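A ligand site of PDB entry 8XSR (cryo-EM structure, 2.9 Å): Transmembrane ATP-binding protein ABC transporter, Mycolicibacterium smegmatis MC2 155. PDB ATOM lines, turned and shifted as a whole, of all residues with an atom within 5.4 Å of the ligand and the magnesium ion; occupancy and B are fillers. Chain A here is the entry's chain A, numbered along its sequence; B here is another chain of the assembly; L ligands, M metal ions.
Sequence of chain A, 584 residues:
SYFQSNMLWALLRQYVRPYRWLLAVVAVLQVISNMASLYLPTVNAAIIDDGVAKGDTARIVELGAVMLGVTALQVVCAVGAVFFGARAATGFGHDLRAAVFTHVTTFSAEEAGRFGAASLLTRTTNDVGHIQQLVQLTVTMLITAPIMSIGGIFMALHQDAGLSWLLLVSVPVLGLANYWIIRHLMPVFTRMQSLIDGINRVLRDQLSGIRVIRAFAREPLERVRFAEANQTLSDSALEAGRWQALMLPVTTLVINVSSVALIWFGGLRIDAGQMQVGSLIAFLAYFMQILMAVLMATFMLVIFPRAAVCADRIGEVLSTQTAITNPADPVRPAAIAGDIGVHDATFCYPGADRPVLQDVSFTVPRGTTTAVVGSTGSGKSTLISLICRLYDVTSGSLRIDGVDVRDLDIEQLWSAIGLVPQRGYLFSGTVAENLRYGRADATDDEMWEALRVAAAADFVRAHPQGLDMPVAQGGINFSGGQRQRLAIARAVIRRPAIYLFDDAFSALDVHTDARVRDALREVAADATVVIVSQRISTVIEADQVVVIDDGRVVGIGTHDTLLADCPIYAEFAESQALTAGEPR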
ATOM      1  N   GLU A 110      10.451 -29.016  15.110  1.00  0.00           N
ATOM      2  CA  GLU A 110       9.284 -29.435  15.884  1.00  0.00           C
ATOM      3  C   GLU A 110       9.084 -30.944  15.812  1.00  0.00           C
ATOM      4  O   GLU A 110       8.856 -31.589  16.837  1.00  0.00           O
ATOM      5  CB  GLU A 110       8.044 -28.708  15.371  1.00  0.00           C
ATOM      6  CG  GLU A 110       6.770 -29.024  16.119  1.00  0.00           C
ATOM      7  CD  GLU A 110       5.578 -28.239  15.607  1.00  0.00           C
ATOM      8  OE1 GLU A 110       5.759 -27.442  14.665  1.00  0.00           O
ATOM      9  OE2 GLU A 110       4.459 -28.437  16.134  1.00  0.00           O
ATOM     10  N   GLY A 113      11.847 -32.692  17.692  1.00  0.00           N
ATOM     11  CA  GLY A 113      11.687 -32.496  19.125  1.00  0.00           C
ATOM     12  C   GLY A 113      10.509 -33.250  19.720  1.00  0.00           C
ATOM     13  O   GLY A 113      10.535 -33.554  20.909  1.00  0.00           O
ATOM     14  N   TYR A 349       1.092 -23.927  18.432  1.00  0.00           N
ATOM     15  CA  TYR A 349       1.221 -25.371  18.326  1.00  0.00           C
ATOM     16  C   TYR A 349      -0.171 -25.986  18.178  1.00  0.00           C
ATOM     17  O   TYR A 349      -1.137 -25.503  18.766  1.00  0.00           O
ATOM     18  CB  TYR A 349       1.936 -25.930  19.556  1.00  0.00           C
ATOM     19  CG  TYR A 349       3.402 -25.603  19.577  1.00  0.00           C
ATOM     20  CD1 TYR A 349       4.317 -26.393  18.898  1.00  0.00           C
ATOM     21  CD2 TYR A 349       3.872 -24.485  20.234  1.00  0.00           C
ATOM     22  CE1 TYR A 349       5.660 -26.086  18.902  1.00  0.00           C
ATOM     23  CE2 TYR A 349       5.216 -24.178  20.238  1.00  0.00           C
ATOM     24  CZ  TYR A 349       6.095 -24.977  19.568  1.00  0.00           C
ATOM     25  OH  TYR A 349       7.428 -24.650  19.583  1.00  0.00           O
ATOM     26  N   VAL A 356       1.908 -19.153  20.720  1.00  0.00           N
ATOM     27  CA  VAL A 356       3.219 -18.748  21.244  1.00  0.00           C
ATOM     28  C   VAL A 356       3.494 -17.294  20.889  1.00  0.00           C
ATOM     29  O   VAL A 356       3.814 -16.475  21.752  1.00  0.00           O
ATOM     30  CB  VAL A 356       4.321 -19.675  20.702  1.00  0.00           C
ATOM     31  CG1 VAL A 356       5.679 -19.166  21.129  1.00  0.00           C
ATOM     32  CG2 VAL A 356       4.105 -21.077  21.208  1.00  0.00           C
ATOM     33  N   SER A 375      10.162 -12.434  28.889  1.00  0.00           N
ATOM     34  CA  SER A 375      10.263 -13.360  30.006  1.00  0.00           C
ATOM     35  C   SER A 375      10.568 -14.773  29.524  1.00  0.00           C
ATOM     36  O   SER A 375      10.906 -14.975  28.361  1.00  0.00           O
ATOM     37  CB  SER A 375       8.964 -13.352  30.828  1.00  0.00           C
ATOM     38  OG  SER A 375       8.756 -12.098  31.430  1.00  0.00           O
ATOM     39  N   THR A 376      10.472 -15.741  30.423  1.00  0.00           N
ATOM     40  CA  THR A 376      10.616 -17.140  30.044  1.00  0.00           C
ATOM     41  C   THR A 376       9.362 -17.615  29.315  1.00  0.00           C
ATOM     42  O   THR A 376       8.234 -17.247  29.682  1.00  0.00           O
ATOM     43  CB  THR A 376      10.891 -18.005  31.272  1.00  0.00           C
ATOM     44  OG1 THR A 376      11.116 -19.356  30.881  1.00  0.00           O
ATOM     45  CG2 THR A 376       9.732 -17.952  32.255  1.00  0.00           C
ATOM     46  N   GLY A 377       9.553 -18.406  28.264  1.00  0.00           N
ATOM     47  CA  GLY A 377       8.444 -18.939  27.515  1.00  0.00           C
ATOM     48  C   GLY A 377       7.574 -17.922  26.824  1.00  0.00           C
ATOM     49  O   GLY A 377       6.382 -18.166  26.630  1.00  0.00           O
ATOM     50  N   SER A 378       8.124 -16.767  26.449  1.00  0.00           N
ATOM     51  CA  SER A 378       7.349 -15.691  25.856  1.00  0.00           C
ATOM     52  C   SER A 378       7.402 -15.672  24.331  1.00  0.00           C
ATOM     53  O   SER A 378       6.719 -14.853  23.716  1.00  0.00           O
ATOM     54  CB  SER A 378       7.810 -14.341  26.409  1.00  0.00           C
ATOM     55  OG  SER A 378       9.131 -14.042  25.985  1.00  0.00           O
ATOM     56  N   GLY A 379       8.195 -16.546  23.720  1.00  0.00           N
ATOM     57  CA  GLY A 379       8.232 -16.671  22.274  1.00  0.00           C
ATOM     58  C   GLY A 379       9.502 -16.176  21.614  1.00  0.00           C
ATOM     59  O   GLY A 379       9.495 -15.961  20.395  1.00  0.00           O
ATOM     60  N   LYS A 380      10.597 -15.996  22.348  1.00  0.00           N
ATOM     61  CA  LYS A 380      11.797 -15.435  21.742  1.00  0.00           C
ATOM     62  C   LYS A 380      12.523 -16.467  20.889  1.00  0.00           C
ATOM     63  O   LYS A 380      12.890 -16.167  19.746  1.00  0.00           O
ATOM     64  CB  LYS A 380      12.733 -14.907  22.829  1.00  0.00           C
ATOM     65  CG  LYS A 380      12.236 -13.687  23.565  1.00  0.00           C
ATOM     66  CD  LYS A 380      13.284 -13.177  24.534  1.00  0.00           C
ATOM     67  CE  LYS A 380      13.063 -13.722  25.923  1.00  0.00           C
ATOM     68  NZ  LYS A 380      13.438 -15.147  26.035  1.00  0.00           N
ATOM     69  N   SER A 381      12.764 -17.657  21.408  1.00  0.00           N
ATOM     70  CA  SER A 381      13.404 -18.708  20.633  1.00  0.00           C
ATOM     71  C   SER A 381      12.515 -19.235  19.527  1.00  0.00           C
ATOM     72  O   SER A 381      13.025 -19.795  18.548  1.00  0.00           O
ATOM     73  CB  SER A 381      13.828 -19.873  21.533  1.00  0.00           C
ATOM     74  OG  SER A 381      14.789 -19.454  22.476  1.00  0.00           O
ATOM     75  N   THR A 382      11.196 -19.089  19.661  1.00  0.00           N
ATOM     76  CA  THR A 382      10.281 -19.426  18.576  1.00  0.00           C
ATOM     77  C   THR A 382      10.350 -18.435  17.432  1.00  0.00           C
ATOM     78  O   THR A 382      10.080 -18.805  16.293  1.00  0.00           O
ATOM     79  CB  THR A 382       8.846 -19.505  19.126  1.00  0.00           C
ATOM     80  OG1 THR A 382       8.796 -20.489  20.161  1.00  0.00           O
ATOM     81  CG2 THR A 382       7.874 -19.898  18.038  1.00  0.00           C
ATOM     82  N   LEU A 383      10.762 -17.195  17.691  1.00  0.00           N
ATOM     83  CA  LEU A 383      10.927 -16.199  16.659  1.00  0.00           C
ATOM     84  C   LEU A 383      12.211 -16.382  15.859  1.00  0.00           C
ATOM     85  O   LEU A 383      12.189 -16.244  14.625  1.00  0.00           O
ATOM     86  CB  LEU A 383      10.896 -14.797  17.280  1.00  0.00           C
ATOM     87  CG  LEU A 383      10.813 -13.573  16.379  1.00  0.00           C
ATOM     88  CD1 LEU A 383       9.490 -13.565  15.641  1.00  0.00           C
ATOM     89  CD2 LEU A 383      10.946 -12.322  17.224  1.00  0.00           C
ATOM     90  N   TYR A 391      10.863 -23.443  12.387  1.00  0.00           N
ATOM     91  CA  TYR A 391       9.423 -23.523  12.525  1.00  0.00           C
ATOM     92  C   TYR A 391       8.796 -22.796  11.345  1.00  0.00           C
ATOM     93  O   TYR A 391       9.466 -22.076  10.613  1.00  0.00           O
ATOM     94  CB  TYR A 391       8.926 -22.908  13.832  1.00  0.00           C
ATOM     95  CG  TYR A 391       9.264 -23.733  15.042  1.00  0.00           C
ATOM     96  CD1 TYR A 391       9.674 -25.048  14.908  1.00  0.00           C
ATOM     97  CD2 TYR A 391       9.150 -23.218  16.315  1.00  0.00           C
ATOM     98  CE1 TYR A 391       9.985 -25.812  16.004  1.00  0.00           C
ATOM     99  CE2 TYR A 391       9.450 -23.973  17.420  1.00  0.00           C
ATOM    100  CZ  TYR A 391       9.869 -25.274  17.259  1.00  0.00           C
ATOM    101  OH  TYR A 391      10.167 -26.048  18.361  1.00  0.00           O
ATOM    102  N   GLN A 422      20.016 -21.382  21.738  1.00  0.00           N
ATOM    103  CA  GLN A 422      20.122 -21.580  23.176  1.00  0.00           C
ATOM    104  C   GLN A 422      20.797 -22.908  23.492  1.00  0.00           C
ATOM    105  O   GLN A 422      21.837 -22.944  24.147  1.00  0.00           O
ATOM    106  CB  GLN A 422      18.744 -21.521  23.846  1.00  0.00           C
ATOM    107  CG  GLN A 422      18.100 -20.166  23.899  1.00  0.00           C
ATOM    108  CD  GLN A 422      16.800 -20.181  24.675  1.00  0.00           C
ATOM    109  OE1 GLN A 422      16.375 -21.223  25.176  1.00  0.00           O
ATOM    110  NE2 GLN A 422      16.153 -19.026  24.771  1.00  0.00           N
ATOM    111  N   ASP A 502      20.665 -16.490  20.071  1.00  0.00           N
ATOM    112  CA  ASP A 502      19.521 -16.887  20.886  1.00  0.00           C
ATOM    113  C   ASP A 502      20.050 -17.247  22.272  1.00  0.00           C
ATOM    114  O   ASP A 502      20.462 -18.373  22.524  1.00  0.00           O
ATOM    115  CB  ASP A 502      18.792 -18.052  20.244  1.00  0.00           C
ATOM    116  CG  ASP A 502      17.476 -18.373  20.917  1.00  0.00           C
ATOM    117  OD1 ASP A 502      17.103 -17.666  21.873  1.00  0.00           O
ATOM    118  OD2 ASP A 502      16.816 -19.336  20.492  1.00  0.00           O
ATOM    119  N   ASP A 503      20.023 -16.269  23.177  1.00  0.00           N
ATOM    120  CA  ASP A 503      20.647 -16.391  24.499  1.00  0.00           C
ATOM    121  C   ASP A 503      22.069 -16.920  24.369  1.00  0.00           C
ATOM    122  O   ASP A 503      22.459 -17.937  24.946  1.00  0.00           O
ATOM    123  CB  ASP A 503      19.796 -17.272  25.419  1.00  0.00           C
ATOM    124  CG  ASP A 503      18.530 -16.587  25.889  1.00  0.00           C
ATOM    125  OD1 ASP A 503      18.543 -15.347  26.005  1.00  0.00           O
ATOM    126  OD2 ASP A 503      17.516 -17.282  26.129  1.00  0.00           O
ATOM    127  N   GLN A 534      17.644 -12.260  27.820  1.00  0.00           N
ATOM    128  CA  GLN A 534      16.966 -11.819  29.028  1.00  0.00           C
ATOM    129  C   GLN A 534      17.753 -10.770  29.795  1.00  0.00           C
ATOM    130  O   GLN A 534      17.198 -10.144  30.698  1.00  0.00           O
ATOM    131  CB  GLN A 534      16.701 -13.015  29.961  1.00  0.00           C
ATOM    132  CG  GLN A 534      15.747 -14.047  29.401  1.00  0.00           C
ATOM    133  CD  GLN A 534      15.638 -15.257  30.291  1.00  0.00           C
ATOM    134  OE1 GLN A 534      16.350 -15.379  31.282  1.00  0.00           O
ATOM    135  NE2 GLN A 534      14.738 -16.163  29.933  1.00  0.00           N
ATOM    136  N   PHE B 509       2.327 -20.180  30.645  1.00  0.00           N
ATOM    137  CA  PHE B 509       2.868 -20.989  29.564  1.00  0.00           C
ATOM    138  C   PHE B 509       2.132 -22.298  29.360  1.00  0.00           C
ATOM    139  O   PHE B 509       2.555 -23.101  28.530  1.00  0.00           O
ATOM    140  CB  PHE B 509       4.355 -21.298  29.790  1.00  0.00           C
ATOM    141  CG  PHE B 509       4.635 -22.230  30.936  1.00  0.00           C
ATOM    142  CD1 PHE B 509       4.975 -21.740  32.175  1.00  0.00           C
ATOM    143  CD2 PHE B 509       4.592 -23.610  30.759  1.00  0.00           C
ATOM    144  CE1 PHE B 509       5.259 -22.595  33.219  1.00  0.00           C
ATOM    145  CE2 PHE B 509       4.854 -24.465  31.807  1.00  0.00           C
ATOM    146  CZ  PHE B 509       5.188 -23.952  33.038  1.00  0.00           C
ATOM    147  N   THR B 512      -0.281 -22.386  26.180  1.00  0.00           N
ATOM    148  CA  THR B 512       0.417 -22.330  24.905  1.00  0.00           C
ATOM    149  C   THR B 512       0.892 -23.737  24.566  1.00  0.00           C
ATOM    150  O   THR B 512       1.526 -23.961  23.535  1.00  0.00           O
ATOM    151  CB  THR B 512       1.583 -21.339  24.962  1.00  0.00           C
ATOM    152  OG1 THR B 512       2.058 -21.076  23.634  1.00  0.00           O
ATOM    153  CG2 THR B 512       2.714 -21.884  25.766  1.00  0.00           C
ATOM    154  N   LEU B 513       0.588 -24.677  25.441  1.00  0.00           N
ATOM    155  CA  LEU B 513       0.844 -26.089  25.218  1.00  0.00           C
ATOM    156  C   LEU B 513      -0.348 -26.724  24.504  1.00  0.00           C
ATOM    157  O   LEU B 513      -1.484 -26.269  24.662  1.00  0.00           O
ATOM    158  CB  LEU B 513       1.090 -26.796  26.546  1.00  0.00           C
ATOM    159  CG  LEU B 513       2.281 -26.301  27.365  1.00  0.00           C
ATOM    160  CD1 LEU B 513       2.360 -26.998  28.700  1.00  0.00           C
ATOM    161  CD2 LEU B 513       3.557 -26.480  26.595  1.00  0.00           C
ATOM    162  N   PRO B 514      -0.114 -27.762  23.701  1.00  0.00           N
ATOM    163  CA  PRO B 514      -1.236 -28.378  22.967  1.00  0.00           C
ATOM    164  C   PRO B 514      -2.376 -28.829  23.860  1.00  0.00           C
ATOM    165  O   PRO B 514      -3.544 -28.520  23.567  1.00  0.00           O
ATOM    166  CB  PRO B 514      -0.572 -29.560  22.243  1.00  0.00           C
ATOM    167  CG  PRO B 514       0.855 -29.167  22.126  1.00  0.00           C
ATOM    168  CD  PRO B 514       1.172 -28.401  23.369  1.00  0.00           C
ATOM    169  N   GLY B 525       6.804 -32.880  24.043  1.00  0.00           N
ATOM    170  CA  GLY B 525       7.646 -32.750  22.882  1.00  0.00           C
ATOM    171  C   GLY B 525       8.765 -31.765  23.114  1.00  0.00           C
ATOM    172  O   GLY B 525       9.073 -30.940  22.254  1.00  0.00           O
ATOM    173  N   GLY B 526       9.390 -31.833  24.298  1.00  0.00           N
ATOM    174  CA  GLY B 526      10.256 -30.749  24.704  1.00  0.00           C
ATOM    175  C   GLY B 526       9.496 -29.488  24.994  1.00  0.00           C
ATOM    176  O   GLY B 526      10.093 -28.407  25.040  1.00  0.00           O
ATOM    177  N   ALA B 527       8.189 -29.600  25.207  1.00  0.00           N
ATOM    178  CA  ALA B 527       7.343 -28.428  25.396  1.00  0.00           C
ATOM    179  C   ALA B 527       7.680 -27.679  26.674  1.00  0.00           C
ATOM    180  O   ALA B 527       7.564 -26.450  26.720  1.00  0.00           O
ATOM    181  CB  ALA B 527       5.874 -28.854  25.423  1.00  0.00           C
ATOM    182  N   ILE B 528       8.096 -28.390  27.713  1.00  0.00           N
ATOM    183  CA  ILE B 528       8.337 -27.791  29.015  1.00  0.00           C
ATOM    184  C   ILE B 528       9.812 -27.460  29.123  1.00  0.00           C
ATOM    185  O   ILE B 528      10.659 -28.369  29.120  1.00  0.00           O
ATOM    186  CB  ILE B 528       7.883 -28.724  30.143  1.00  0.00           C
ATOM    187  CG1 ILE B 528       6.403 -29.084  29.966  1.00  0.00           C
ATOM    188  CG2 ILE B 528       8.042 -28.054  31.474  1.00  0.00           C
ATOM    189  CD1 ILE B 528       5.953 -30.227  30.834  1.00  0.00           C
ATOM    190  N   SER B 529      10.128 -26.175  29.215  1.00  0.00           N
ATOM    191  CA  SER B 529      11.499 -25.716  29.334  1.00  0.00           C
ATOM    192  C   SER B 529      12.097 -26.153  30.665  1.00  0.00           C
ATOM    193  O   SER B 529      11.432 -26.749  31.512  1.00  0.00           O
ATOM    194  CB  SER B 529      11.548 -24.193  29.198  1.00  0.00           C
ATOM    195  OG  SER B 529      12.857 -23.708  29.366  1.00  0.00           O
ATOM    196  N   GLU B 532      10.696 -23.758  33.106  1.00  0.00           N
ATOM    197  CA  GLU B 532       9.284 -24.022  33.299  1.00  0.00           C
ATOM    198  C   GLU B 532       9.021 -25.230  34.178  1.00  0.00           C
ATOM    199  O   GLU B 532       7.964 -25.286  34.806  1.00  0.00           O
ATOM    200  CB  GLU B 532       8.592 -24.215  31.941  1.00  0.00           C
ATOM    201  CG  GLU B 532       8.592 -22.964  31.090  1.00  0.00           C
ATOM    202  CD  GLU B 532       7.971 -23.182  29.728  1.00  0.00           C
ATOM    203  OE1 GLU B 532       7.680 -24.347  29.398  1.00  0.00           O
ATOM    204  OE2 GLU B 532       7.764 -22.192  28.999  1.00  0.00           O
ATOM    205  N   SER B 557      16.643 -20.744  36.418  1.00  0.00           N
ATOM    206  CA  SER B 557      16.557 -20.986  34.993  1.00  0.00           C
ATOM    207  C   SER B 557      15.422 -20.212  34.338  1.00  0.00           C
ATOM    208  O   SER B 557      15.055 -20.515  33.202  1.00  0.00           O
ATOM    209  CB  SER B 557      16.362 -22.481  34.714  1.00  0.00           C
ATOM    210  OG  SER B 557      17.500 -23.239  35.089  1.00  0.00           O
HETATM  211  P1  LIG L   1      13.538 -18.702  27.432  1.00  0.00           P
HETATM  212  O1  LIG L   1      13.711 -17.229  27.669  1.00  0.00           O
HETATM  213  O2  LIG L   1      14.502 -19.276  26.420  1.00  0.00           O
HETATM  214  O3  LIG L   1      13.400 -19.550  28.661  1.00  0.00           O
HETATM  215  P2  LIG L   1      11.853 -18.417  25.194  1.00  0.00           P
HETATM  216  O4  LIG L   1      12.809 -19.179  24.331  1.00  0.00           O
HETATM  217  O5  LIG L   1      11.767 -16.926  25.120  1.00  0.00           O
HETATM  218  O6  LIG L   1      12.100 -18.823  26.725  1.00  0.00           O
HETATM  219  P3  LIG L   1       9.994 -20.041  23.798  1.00  0.00           P
HETATM  220  O7  LIG L   1      10.790 -21.300  23.960  1.00  0.00           O
HETATM  221  O8  LIG L   1       9.997 -19.312  22.481  1.00  0.00           O
HETATM  222  O9  LIG L   1      10.369 -19.014  24.971  1.00  0.00           O
HETATM  223  O10 LIG L   1       8.470 -20.363  24.192  1.00  0.00           O
HETATM  224  C1  LIG L   1       7.670 -21.198  23.369  1.00  0.00           C
HETATM  225  C2  LIG L   1       6.453 -21.666  24.153  1.00  0.00           C
HETATM  226  O11 LIG L   1       5.883 -22.770  23.450  1.00  0.00           O
HETATM  227  C3  LIG L   1       6.848 -22.147  25.525  1.00  0.00           C
HETATM  228  O12 LIG L   1       6.042 -21.509  26.517  1.00  0.00           O
HETATM  229  C4  LIG L   1       6.585 -23.637  25.543  1.00  0.00           C
HETATM  230  O13 LIG L   1       5.735 -23.960  26.652  1.00  0.00           O
HETATM  231  C5  LIG L   1       5.898 -23.960  24.231  1.00  0.00           C
HETATM  232  N1  LIG L   1       6.676 -24.985  23.499  1.00  0.00           N
HETATM  233  C6  LIG L   1       8.000 -24.952  23.268  1.00  0.00           C
HETATM  234  N2  LIG L   1       8.411 -26.039  22.559  1.00  0.00           N
HETATM  235  C7  LIG L   1       7.324 -26.794  22.340  1.00  0.00           C
HETATM  236  C8  LIG L   1       7.047 -28.076  21.671  1.00  0.00           C
HETATM  237  N3  LIG L   1       8.032 -28.783  21.076  1.00  0.00           N
HETATM  238  N4  LIG L   1       5.772 -28.520  21.666  1.00  0.00           N
HETATM  239  C9  LIG L   1       4.777 -27.822  22.256  1.00  0.00           C
HETATM  240  N5  LIG L   1       4.957 -26.650  22.892  1.00  0.00           N
HETATM  241  C10 LIG L   1       6.185 -26.093  22.964  1.00  0.00           C
HETATM  242 MG    MG M   1      14.497 -20.457  24.143  1.00  0.00          MG
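CG2 of Val 356 touches O11 of the ligand, 3.3 Å away.
Ser 375 touches the ligand.
Ser 378 touches the ligand (N to O9, 3.5 Å).
CA of Gly 379 touches O8 of the ligand, at 3.2 Å.
OD2 of Asp 503 touches O2 of the ligand, 3.6 Å away.
Phe 509 of chain B touches the ligand (CB to O12, 3.7 Å).
CG2 of Thr 512 of chain B touches O12 of the ligand, at 3.4 Å.
CD2 of Leu 513 of chain B touches O13 of the ligand, 3.3 Å away.
Pro 514 of chain B touches the ligand.
Gly 526 of chain B touches the ligand (O to N2, 3.8 Å).
Hydrophobic or aromatic side chains within 4 Å of the ligand: Tyr 349, Val 356, Phe 509 of chain B, Leu 513 of chain B, Pro 514 of chain B and Ala 527 of chain B.
Along chain A the residues within 4 Å of the ligand span positions 349 to 534.
The backbone NH (N) of Ser 381 sits at hydrogen-bond distance from an oxygen (O8) of the ligand, at 3.4 Å.
N of Lys 380 is in hydrogen-bond range of O5 of the ligand, 3.1 Å away.
The side-chain amino group of Lys 380 is in salt-bridge range of an oxygen (O5) of the ligand, at 2.6 Å.
N3 of the ligand lies within hydrogen-bond range of O of Gly 525 of chain B (2.7 Å).
O1 of the ligand is in hydrogen-bond range of NE2 of Gln 534 (2.7 Å).
N of Thr 382 sits at hydrogen-bond distance from O8 of the ligand (3.1 Å).
O8 of the ligand is in hydrogen-bond range of OG1 of Thr 382, at 2.9 Å.
The backbone NH of Gly 377 lies within hydrogen-bond range of an oxygen (O6) of the ligand (3.0 Å).
The backbone carbonyl oxygen (O) of Gly 377 lies within hydrogen-bond range of an oxygen (O12) of the ligand, at 3.4 Å.
The backbone carbonyl oxygen of Ala 527 of chain B lies within hydrogen-bond range of an oxygen (O13) of the ligand (3.1 Å).
O12 of the ligand sits at hydrogen-bond distance from OE2 of Glu 532 of chain B (3.1 Å).
An oxygen (O3) of the ligand sits at hydrogen-bond distance from the side-chain hydroxyl of Thr 376, 3.2 Å away.
The side-chain hydroxyl (OH) of Tyr 349 is in hydrogen-bond range of a nitrogen (N2) of the ligand (3.4 Å).
The magnesium ion is bound by the side-chain hydroxyl of Ser 381 (2.0 Å), an oxygen (O4) of the ligand (2.1 Å), the side-chain amide oxygen of Gln 422 (2.3 Å), the side-chain amide nitrogen of Gln 422 (2.3 Å) and an oxygen (O2) of the ligand (2.6 Å).
The side-chain hydroxyl (OG) of Ser 381 sits close to the side-chain carboxylate (OD2) of Asp 502 (2.8 Å).
The side-chain amide nitrogen (NE2) of Gln 422 sits close to the side-chain carboxylate (OD2) of Asp 503, at 2.6 Å.
N of Gln 422 sits at hydrogen-bond distance from O of Asp 502 (3.1 Å).
The backbone carbonyl oxygen of Ser 375 lies within hydrogen-bond range of the side-chain amino group of Lys 380, 3.4 Å away.
OE1 of Glu 532 of chain B is in hydrogen-bond range of N of Ser 529 of chain B (3.1 Å).
N of Val 356 sits close to OG1 of Thr 512 of chain B, 3.5 Å away.
OH of Tyr 391 lies close to OH of Tyr 349 (3.3 Å).
O of Ser 375 is in hydrogen-bond range of OG of Ser 378, 3.1 Å away.
Within 4 Å of the magnesium ion: Ser 381 and Gln 422.
The nearest printed residue that does not touch the magnesium ion is Asp 502 (4.4 Å).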
